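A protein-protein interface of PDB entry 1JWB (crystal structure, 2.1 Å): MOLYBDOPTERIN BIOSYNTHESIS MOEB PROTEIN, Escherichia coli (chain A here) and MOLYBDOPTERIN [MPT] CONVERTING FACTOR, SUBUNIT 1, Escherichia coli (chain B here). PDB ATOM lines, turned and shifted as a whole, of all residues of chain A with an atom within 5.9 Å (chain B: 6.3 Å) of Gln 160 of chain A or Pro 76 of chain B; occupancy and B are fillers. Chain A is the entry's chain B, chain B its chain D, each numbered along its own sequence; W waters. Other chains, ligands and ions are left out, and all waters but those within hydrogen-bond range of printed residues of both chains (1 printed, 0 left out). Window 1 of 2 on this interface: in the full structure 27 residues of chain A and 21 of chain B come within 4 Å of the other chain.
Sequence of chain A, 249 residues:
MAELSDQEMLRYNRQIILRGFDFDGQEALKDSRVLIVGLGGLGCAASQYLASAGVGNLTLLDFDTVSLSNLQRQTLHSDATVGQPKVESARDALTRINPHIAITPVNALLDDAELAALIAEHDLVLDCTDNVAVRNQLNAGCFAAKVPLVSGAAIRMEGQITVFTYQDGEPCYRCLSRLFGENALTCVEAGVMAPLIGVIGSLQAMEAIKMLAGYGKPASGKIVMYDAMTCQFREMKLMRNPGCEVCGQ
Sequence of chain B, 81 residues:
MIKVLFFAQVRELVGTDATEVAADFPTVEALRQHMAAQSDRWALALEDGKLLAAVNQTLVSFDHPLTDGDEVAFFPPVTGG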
ATOM      1  N   SER A 151      18.665 -25.816 -12.901  1.00  0.00           N
ATOM      2  CA  SER A 151      19.930 -25.355 -13.360  1.00  0.00           C
ATOM      3  C   SER A 151      20.891 -25.249 -12.214  1.00  0.00           C
ATOM      4  O   SER A 151      20.642 -24.578 -11.227  1.00  0.00           O
ATOM      5  CB  SER A 151      19.741 -23.957 -13.939  1.00  0.00           C
ATOM      6  OG  SER A 151      20.883 -23.504 -14.626  1.00  0.00           O
ATOM      7  N   GLY A 152      21.993 -25.962 -12.351  1.00  0.00           N
ATOM      8  CA  GLY A 152      22.999 -25.935 -11.336  1.00  0.00           C
ATOM      9  C   GLY A 152      24.326 -25.575 -11.934  1.00  0.00           C
ATOM     10  O   GLY A 152      24.613 -25.932 -13.070  1.00  0.00           O
ATOM     11  N   ALA A 153      25.154 -24.890 -11.146  1.00  0.00           N
ATOM     12  CA  ALA A 153      26.458 -24.605 -11.597  1.00  0.00           C
ATOM     13  C   ALA A 153      27.399 -24.647 -10.422  1.00  0.00           C
ATOM     14  O   ALA A 153      27.038 -24.308  -9.282  1.00  0.00           O
ATOM     15  CB  ALA A 153      26.453 -23.174 -12.287  1.00  0.00           C
ATOM     16  N   ALA A 154      28.641 -24.996 -10.703  1.00  0.00           N
ATOM     17  CA  ALA A 154      29.657 -25.063  -9.667  1.00  0.00           C
ATOM     18  C   ALA A 154      30.988 -24.925 -10.297  1.00  0.00           C
ATOM     19  O   ALA A 154      31.246 -25.493 -11.349  1.00  0.00           O
ATOM     20  CB  ALA A 154      29.596 -26.421  -8.955  1.00  0.00           C
ATOM     21  N   GLU A 158      32.255 -22.105  -5.335  1.00  0.00           N
ATOM     22  CA  GLU A 158      31.037 -21.362  -5.514  1.00  0.00           C
ATOM     23  C   GLU A 158      30.053 -22.200  -6.274  1.00  0.00           C
ATOM     24  O   GLU A 158      30.362 -22.706  -7.321  1.00  0.00           O
ATOM     25  CB  GLU A 158      31.256 -20.061  -6.308  1.00  0.00           C
ATOM     26  CG  GLU A 158      30.020 -19.195  -6.281  1.00  0.00           C
ATOM     27  CD  GLU A 158      30.099 -18.008  -7.207  1.00  0.00           C
ATOM     28  OE1 GLU A 158      31.197 -17.724  -7.677  1.00  0.00           O
ATOM     29  OE2 GLU A 158      29.039 -17.397  -7.503  1.00  0.00           O
ATOM     30  N   GLY A 159      28.850 -22.298  -5.749  1.00  0.00           N
ATOM     31  CA  GLY A 159      27.803 -22.981  -6.460  1.00  0.00           C
ATOM     32  C   GLY A 159      26.541 -22.161  -6.567  1.00  0.00           C
ATOM     33  O   GLY A 159      26.325 -21.201  -5.842  1.00  0.00           O
ATOM     34  N   GLN A 160      25.692 -22.539  -7.499  1.00  0.00           N
ATOM     35  CA  GLN A 160      24.477 -21.823  -7.688  1.00  0.00           C
ATOM     36  C   GLN A 160      23.440 -22.724  -8.217  1.00  0.00           C
ATOM     37  O   GLN A 160      23.716 -23.610  -9.038  1.00  0.00           O
ATOM     38  CB  GLN A 160      24.652 -20.758  -8.762  1.00  0.00           C
ATOM     39  CG  GLN A 160      25.201 -19.466  -8.265  1.00  0.00           C
ATOM     40  CD  GLN A 160      25.535 -18.514  -9.417  1.00  0.00           C
ATOM     41  OE1 GLN A 160      24.919 -18.577 -10.484  1.00  0.00           O
ATOM     42  NE2 GLN A 160      26.515 -17.642  -9.195  1.00  0.00           N
ATOM     43  N   ILE A 161      22.235 -22.414  -7.807  1.00  0.00           N
ATOM     44  CA  ILE A 161      21.075 -23.061  -8.333  1.00  0.00           C
ATOM     45  C   ILE A 161      19.891 -22.134  -8.603  1.00  0.00           C
ATOM     46  O   ILE A 161      19.609 -21.203  -7.848  1.00  0.00           O
ATOM     47  CB  ILE A 161      20.641 -24.193  -7.418  1.00  0.00           C
ATOM     48  CG1 ILE A 161      19.221 -24.618  -7.762  1.00  0.00           C
ATOM     49  CG2 ILE A 161      20.858 -23.934  -5.954  1.00  0.00           C
ATOM     50  CD1 ILE A 161      18.887 -26.064  -7.462  1.00  0.00           C
ATOM     51  N   THR A 162      19.223 -22.422  -9.719  1.00  0.00           N
ATOM     52  CA  THR A 162      17.948 -21.798 -10.045  1.00  0.00           C
ATOM     53  C   THR A 162      17.018 -22.799 -10.674  1.00  0.00           C
ATOM     54  O   THR A 162      17.450 -23.654 -11.447  1.00  0.00           O
ATOM     55  CB  THR A 162      18.111 -20.689 -11.078  1.00  0.00           C
ATOM     56  OG1 THR A 162      18.829 -19.590 -10.503  1.00  0.00           O
ATOM     57  CG2 THR A 162      16.745 -20.087 -11.420  1.00  0.00           C
ATOM     58  N   LEU A 176      19.428 -14.231 -17.012  1.00  0.00           N
ATOM     59  CA  LEU A 176      20.639 -14.272 -16.197  1.00  0.00           C
ATOM     60  C   LEU A 176      21.888 -14.258 -17.034  1.00  0.00           C
ATOM     61  O   LEU A 176      22.809 -13.507 -16.751  1.00  0.00           O
ATOM     62  CB  LEU A 176      20.654 -15.509 -15.280  1.00  0.00           C
ATOM     63  CG  LEU A 176      21.975 -15.886 -14.577  1.00  0.00           C
ATOM     64  CD1 LEU A 176      22.571 -14.737 -13.785  1.00  0.00           C
ATOM     65  CD2 LEU A 176      21.826 -17.116 -13.656  1.00  0.00           C
ATOM     66  N   ILE A 200      25.532 -28.783  -4.597  1.00  0.00           N
ATOM     67  CA  ILE A 200      24.680 -28.238  -5.613  1.00  0.00           C
ATOM     68  C   ILE A 200      23.883 -29.322  -6.343  1.00  0.00           C
ATOM     69  O   ILE A 200      22.718 -29.150  -6.687  1.00  0.00           O
ATOM     70  CB  ILE A 200      25.516 -27.404  -6.620  1.00  0.00           C
ATOM     71  CG1 ILE A 200      26.113 -26.179  -5.959  1.00  0.00           C
ATOM     72  CG2 ILE A 200      24.635 -26.949  -7.743  1.00  0.00           C
ATOM     73  CD1 ILE A 200      25.063 -25.347  -5.191  1.00  0.00           C
ATOM     74  N   ILE A 223      18.562 -16.798  -7.607  1.00  0.00           N
ATOM     75  CA  ILE A 223      19.784 -17.588  -7.710  1.00  0.00           C
ATOM     76  C   ILE A 223      20.080 -17.879  -6.260  1.00  0.00           C
ATOM     77  O   ILE A 223      20.145 -16.937  -5.448  1.00  0.00           O
ATOM     78  CB  ILE A 223      21.002 -16.782  -8.240  1.00  0.00           C
ATOM     79  CG1 ILE A 223      20.915 -16.480  -9.711  1.00  0.00           C
ATOM     80  CG2 ILE A 223      22.264 -17.539  -8.057  1.00  0.00           C
ATOM     81  CD1 ILE A 223      22.168 -15.778 -10.205  1.00  0.00           C
ATOM     82  N   VAL A 224      20.240 -19.151  -5.924  1.00  0.00           N
ATOM     83  CA  VAL A 224      20.708 -19.532  -4.606  1.00  0.00           C
ATOM     84  C   VAL A 224      22.181 -19.712  -4.841  1.00  0.00           C
ATOM     85  O   VAL A 224      22.577 -20.448  -5.711  1.00  0.00           O
ATOM     86  CB  VAL A 224      20.075 -20.832  -4.109  1.00  0.00           C
ATOM     87  CG1 VAL A 224      20.632 -21.246  -2.751  1.00  0.00           C
ATOM     88  CG2 VAL A 224      18.588 -20.717  -4.041  1.00  0.00           C
ATOM     89  N   MET A 225      22.979 -18.966  -4.098  1.00  0.00           N
ATOM     90  CA  MET A 225      24.431 -18.955  -4.279  1.00  0.00           C
ATOM     91  C   MET A 225      25.021 -19.455  -2.985  1.00  0.00           C
ATOM     92  O   MET A 225      24.617 -19.058  -1.922  1.00  0.00           O
ATOM     93  CB  MET A 225      24.913 -17.550  -4.589  1.00  0.00           C
ATOM     94  CG  MET A 225      26.308 -17.453  -5.080  1.00  0.00           C
ATOM     95  SD  MET A 225      27.519 -17.561  -3.798  1.00  0.00           S
ATOM     96  CE  MET A 225      27.307 -16.034  -3.064  1.00  0.00           C
ATOM     97  N   TYR A 226      25.928 -20.392  -3.113  1.00  0.00           N
ATOM     98  CA  TYR A 226      26.554 -21.045  -1.983  1.00  0.00           C
ATOM     99  C   TYR A 226      28.002 -20.718  -2.096  1.00  0.00           C
ATOM    100  O   TYR A 226      28.664 -21.023  -3.110  1.00  0.00           O
ATOM    101  CB  TYR A 226      26.390 -22.560  -2.107  1.00  0.00           C
ATOM    102  CG  TYR A 226      27.285 -23.408  -1.258  1.00  0.00           C
ATOM    103  CD1 TYR A 226      27.548 -23.092   0.067  1.00  0.00           C
ATOM    104  CD2 TYR A 226      27.854 -24.549  -1.780  1.00  0.00           C
ATOM    105  CE1 TYR A 226      28.340 -23.889   0.832  1.00  0.00           C
ATOM    106  CE2 TYR A 226      28.657 -25.340  -1.024  1.00  0.00           C
ATOM    107  CZ  TYR A 226      28.901 -25.022   0.278  1.00  0.00           C
ATOM    108  OH  TYR A 226      29.766 -25.802   1.007  1.00  0.00           O
ATOM    109  N   PHE B   7      31.481 -11.518  -2.797  1.00  0.00           N
ATOM    110  CA  PHE B   7      31.277 -12.911  -2.454  1.00  0.00           C
ATOM    111  C   PHE B   7      32.191 -13.802  -3.272  1.00  0.00           C
ATOM    112  O   PHE B   7      32.677 -13.388  -4.335  1.00  0.00           O
ATOM    113  CB  PHE B   7      29.804 -13.283  -2.616  1.00  0.00           C
ATOM    114  CG  PHE B   7      28.941 -12.791  -1.480  1.00  0.00           C
ATOM    115  CD1 PHE B   7      28.178 -11.648  -1.614  1.00  0.00           C
ATOM    116  CD2 PHE B   7      28.914 -13.482  -0.265  1.00  0.00           C
ATOM    117  CE1 PHE B   7      27.390 -11.196  -0.570  1.00  0.00           C
ATOM    118  CE2 PHE B   7      28.128 -13.042   0.777  1.00  0.00           C
ATOM    119  CZ  PHE B   7      27.360 -11.903   0.623  1.00  0.00           C
ATOM    120  N   ALA B   8      32.465 -14.971  -2.682  1.00  0.00           N
ATOM    121  CA  ALA B   8      33.235 -16.041  -3.261  1.00  0.00           C
ATOM    122  C   ALA B   8      34.518 -15.561  -3.863  1.00  0.00           C
ATOM    123  O   ALA B   8      35.296 -14.873  -3.252  1.00  0.00           O
ATOM    124  CB  ALA B   8      32.428 -16.774  -4.262  1.00  0.00           C
ATOM    125  N   GLN B   9      34.779 -15.933  -5.095  1.00  0.00           N
ATOM    126  CA  GLN B   9      36.047 -15.540  -5.625  1.00  0.00           C
ATOM    127  C   GLN B   9      36.301 -14.000  -5.612  1.00  0.00           C
ATOM    128  O   GLN B   9      37.447 -13.557  -5.483  1.00  0.00           O
ATOM    129  CB  GLN B   9      36.216 -16.121  -7.022  1.00  0.00           C
ATOM    130  CG  GLN B   9      37.657 -16.010  -7.537  1.00  0.00           C
ATOM    131  CD  GLN B   9      37.764 -16.045  -9.059  1.00  0.00           C
ATOM    132  OE1 GLN B   9      36.775 -15.785  -9.773  1.00  0.00           O
ATOM    133  NE2 GLN B   9      38.959 -16.371  -9.566  1.00  0.00           N
ATOM    134  N   VAL B  10      35.267 -13.173  -5.789  1.00  0.00           N
ATOM    135  CA  VAL B  10      35.480 -11.723  -5.778  1.00  0.00           C
ATOM    136  C   VAL B  10      36.157 -11.406  -4.437  1.00  0.00           C
ATOM    137  O   VAL B  10      37.222 -10.831  -4.414  1.00  0.00           O
ATOM    138  CB  VAL B  10      34.173 -10.906  -6.002  1.00  0.00           C
ATOM    139  CG1 VAL B  10      34.429  -9.394  -5.976  1.00  0.00           C
ATOM    140  CG2 VAL B  10      33.568 -11.277  -7.362  1.00  0.00           C
ATOM    141  N   ALA B  45      39.111  -9.298 -10.333  1.00  0.00           N
ATOM    142  CA  ALA B  45      37.961  -9.698  -9.553  1.00  0.00           C
ATOM    143  C   ALA B  45      36.694  -9.120 -10.100  1.00  0.00           C
ATOM    144  O   ALA B  45      35.695  -9.837 -10.221  1.00  0.00           O
ATOM    145  CB  ALA B  45      38.130  -9.296  -8.115  1.00  0.00           C
ATOM    146  N   LYS B  50      32.940 -11.244 -16.282  1.00  0.00           N
ATOM    147  CA  LYS B  50      33.171 -12.300 -15.294  1.00  0.00           C
ATOM    148  C   LYS B  50      32.601 -11.869 -13.930  1.00  0.00           C
ATOM    149  O   LYS B  50      33.171 -12.149 -12.861  1.00  0.00           O
ATOM    150  CB  LYS B  50      34.672 -12.569 -15.166  1.00  0.00           C
ATOM    151  CG  LYS B  50      35.315 -13.226 -16.413  1.00  0.00           C
ATOM    152  CD  LYS B  50      36.815 -12.875 -16.479  1.00  0.00           C
ATOM    153  CE  LYS B  50      37.693 -14.021 -16.956  1.00  0.00           C
ATOM    154  NZ  LYS B  50      39.032 -13.945 -16.286  1.00  0.00           N
ATOM    155  N   LEU B  51      31.462 -11.189 -13.968  1.00  0.00           N
ATOM    156  CA  LEU B  51      30.901 -10.628 -12.766  1.00  0.00           C
ATOM    157  C   LEU B  51      29.389 -10.470 -12.760  1.00  0.00           C
ATOM    158  O   LEU B  51      28.733 -10.264 -13.767  1.00  0.00           O
ATOM    159  CB  LEU B  51      31.545  -9.260 -12.540  1.00  0.00           C
ATOM    160  CG  LEU B  51      31.119  -8.426 -11.368  1.00  0.00           C
ATOM    161  CD1 LEU B  51      31.538  -9.095 -10.062  1.00  0.00           C
ATOM    162  CD2 LEU B  51      31.769  -7.064 -11.471  1.00  0.00           C
ATOM    163  N   LEU B  52      28.825 -10.545 -11.584  1.00  0.00           N
ATOM    164  CA  LEU B  52      27.419 -10.385 -11.481  1.00  0.00           C
ATOM    165  C   LEU B  52      27.217  -9.394 -10.404  1.00  0.00           C
ATOM    166  O   LEU B  52      27.979  -9.370  -9.475  1.00  0.00           O
ATOM    167  CB  LEU B  52      26.756 -11.691 -11.047  1.00  0.00           C
ATOM    168  CG  LEU B  52      26.371 -12.695 -12.123  1.00  0.00           C
ATOM    169  CD1 LEU B  52      25.646 -13.857 -11.436  1.00  0.00           C
ATOM    170  CD2 LEU B  52      25.488 -12.058 -13.145  1.00  0.00           C
ATOM    171  N   PHE B  74      28.817  -7.877  -5.389  1.00  0.00           N
ATOM    172  CA  PHE B  74      29.581  -8.302  -6.525  1.00  0.00           C
ATOM    173  C   PHE B  74      29.992  -9.745  -6.317  1.00  0.00           C
ATOM    174  O   PHE B  74      30.478 -10.123  -5.258  1.00  0.00           O
ATOM    175  CB  PHE B  74      30.802  -7.403  -6.671  1.00  0.00           C
ATOM    176  CG  PHE B  74      30.494  -6.087  -7.300  1.00  0.00           C
ATOM    177  CD1 PHE B  74      30.769  -4.902  -6.633  1.00  0.00           C
ATOM    178  CD2 PHE B  74      29.915  -6.040  -8.565  1.00  0.00           C
ATOM    179  CE1 PHE B  74      30.487  -3.689  -7.228  1.00  0.00           C
ATOM    180  CE2 PHE B  74      29.614  -4.845  -9.149  1.00  0.00           C
ATOM    181  CZ  PHE B  74      29.906  -3.646  -8.466  1.00  0.00           C
ATOM    182  N   PHE B  75      29.759 -10.573  -7.311  1.00  0.00           N
ATOM    183  CA  PHE B  75      30.153 -11.943  -7.148  1.00  0.00           C
ATOM    184  C   PHE B  75      30.169 -12.583  -8.497  1.00  0.00           C
ATOM    185  O   PHE B  75      29.627 -12.047  -9.455  1.00  0.00           O
ATOM    186  CB  PHE B  75      29.242 -12.647  -6.165  1.00  0.00           C
ATOM    187  CG  PHE B  75      27.858 -12.824  -6.659  1.00  0.00           C
ATOM    188  CD1 PHE B  75      27.476 -14.014  -7.249  1.00  0.00           C
ATOM    189  CD2 PHE B  75      26.943 -11.789  -6.567  1.00  0.00           C
ATOM    190  CE1 PHE B  75      26.188 -14.184  -7.724  1.00  0.00           C
ATOM    191  CE2 PHE B  75      25.651 -11.944  -7.049  1.00  0.00           C
ATOM    192  CZ  PHE B  75      25.267 -13.132  -7.619  1.00  0.00           C
ATOM    193  N   PRO B  76      30.843 -13.715  -8.596  1.00  0.00           N
ATOM    194  CA  PRO B  76      30.995 -14.346  -9.883  1.00  0.00           C
ATOM    195  C   PRO B  76      29.764 -15.130 -10.296  1.00  0.00           C
ATOM    196  O   PRO B  76      29.051 -15.734  -9.506  1.00  0.00           O
ATOM    197  CB  PRO B  76      32.162 -15.296  -9.654  1.00  0.00           C
ATOM    198  CG  PRO B  76      32.708 -14.931  -8.283  1.00  0.00           C
ATOM    199  CD  PRO B  76      31.560 -14.459  -7.538  1.00  0.00           C
ATOM    200  N   PRO B  77      29.538 -15.113 -11.576  1.00  0.00           N
ATOM    201  CA  PRO B  77      28.590 -16.038 -12.175  1.00  0.00           C
ATOM    202  C   PRO B  77      29.353 -17.331 -12.216  1.00  0.00           C
ATOM    203  O   PRO B  77      30.548 -17.339 -12.046  1.00  0.00           O
ATOM    204  CB  PRO B  77      28.453 -15.571 -13.630  1.00  0.00           C
ATOM    205  CG  PRO B  77      29.660 -14.691 -13.892  1.00  0.00           C
ATOM    206  CD  PRO B  77      30.226 -14.266 -12.559  1.00  0.00           C
ATOM    207  N   VAL B  78      28.668 -18.395 -12.518  1.00  0.00           N
ATOM    208  CA  VAL B  78      29.289 -19.691 -12.557  1.00  0.00           C
ATOM    209  C   VAL B  78      28.589 -20.487 -13.598  1.00  0.00           C
ATOM    210  O   VAL B  78      27.351 -20.554 -13.604  1.00  0.00           O
ATOM    211  CB  VAL B  78      29.163 -20.372 -11.213  1.00  0.00           C
ATOM    212  CG1 VAL B  78      29.501 -21.891 -11.330  1.00  0.00           C
ATOM    213  CG2 VAL B  78      30.062 -19.682 -10.248  1.00  0.00           C
HETATM  214  O   HOH W   1      33.935 -18.116  -7.389  1.00  0.00           O
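The side-chain carboxylate (OE2) of Glu 158 of chain A lies close to the backbone carbonyl oxygen (O) of Pro 76 of chain B, at 2.6 Å.
The side-chain amide nitrogen of Gln 160 of chain A sits at hydrogen-bond distance from the backbone carbonyl oxygen of Pro 76 of chain B (3.2 Å).
The backbone carbonyl oxygen of Ala 153 of chain A sits at hydrogen-bond distance from the backbone NH of Gln 160 of chain A, 2.8 Å away.
The side-chain carboxylate (OE2) of Glu 158 of chain A sits at hydrogen-bond distance from the side-chain amide nitrogen (NE2) of Gln 160 of chain A.
The backbone NH (N) of Phe 7 of chain B is in hydrogen-bond range of the backbone carbonyl oxygen (O) of Phe 74 of chain B, 3.0 Å away.
The backbone NH of Leu 52 of chain B sits at hydrogen-bond distance from the backbone carbonyl oxygen of Phe 75 of chain B (2.7 Å).
Printed residues of chain A that touch a printed residue of chain B: Ala 153, Ala 154, Glu 158, Gln 160, Leu 176 and Met 225.
Hydrophobic or aromatic side chains of chain A within 4 Å of the printed part of chain B: Ala 153, Leu 176 and Met 225.
Of the 13 printed residues of chain B, 7 touch a printed residue of chain A.
Hydrophobic or aromatic side chains of chain B within 4 Å of the printed part of chain A: Phe 7, Ala 8, Leu 52, Phe 75, Pro 76 and Val 78.
Water W1 bridges the side-chain carboxylate of Glu 158 of chain A (2.8 Å) and the backbone NH of Gln 9 of chain B (3.3 Å).
Printed residues of chain B within 4 Å of Ala 154 of chain A: Val 78 (3.3 Å).
Of the printed residues of chain B, Glu 158 of chain A touches Ala 8, Phe 75, Pro 76 and Val 78.
Val 224 of chain A touches none of the printed residues of chain B.
Printed residues of chain A within 4 Å of Leu 52 of chain B: Leu 176 (3.97 Å).
Printed residues of chain A within 4 Å of Phe 75 of chain B: Glu 158 and Gln 160.
Of the printed residues of chain A, Pro 76 of chain B touches Glu 158 (2.6 Å) and Gln 160 (3.2 Å).
The nearest printed residue of chain A that does not touch Val 78 of chain B is Gln 160 of chain A (4.03 Å).
Among the printed residues, pairs that only touch across the chains: Ala 153 of chain A with Val 78 of chain B, Ala 154 of chain A with Val 78 of chain B, Glu 158 of chain A with Ala 8 of chain B, Glu 158 of chain A with Phe 75 of chain B, Glu 158 of chain A with Val 78 of chain B, Gln 160 of chain A with Phe 75 of chain B, Gln 160 of chain A with Pro 77 of chain B, Leu 176 of chain A with Leu 52 of chain B and Met 225 of chain A with Phe 7 of chain B.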
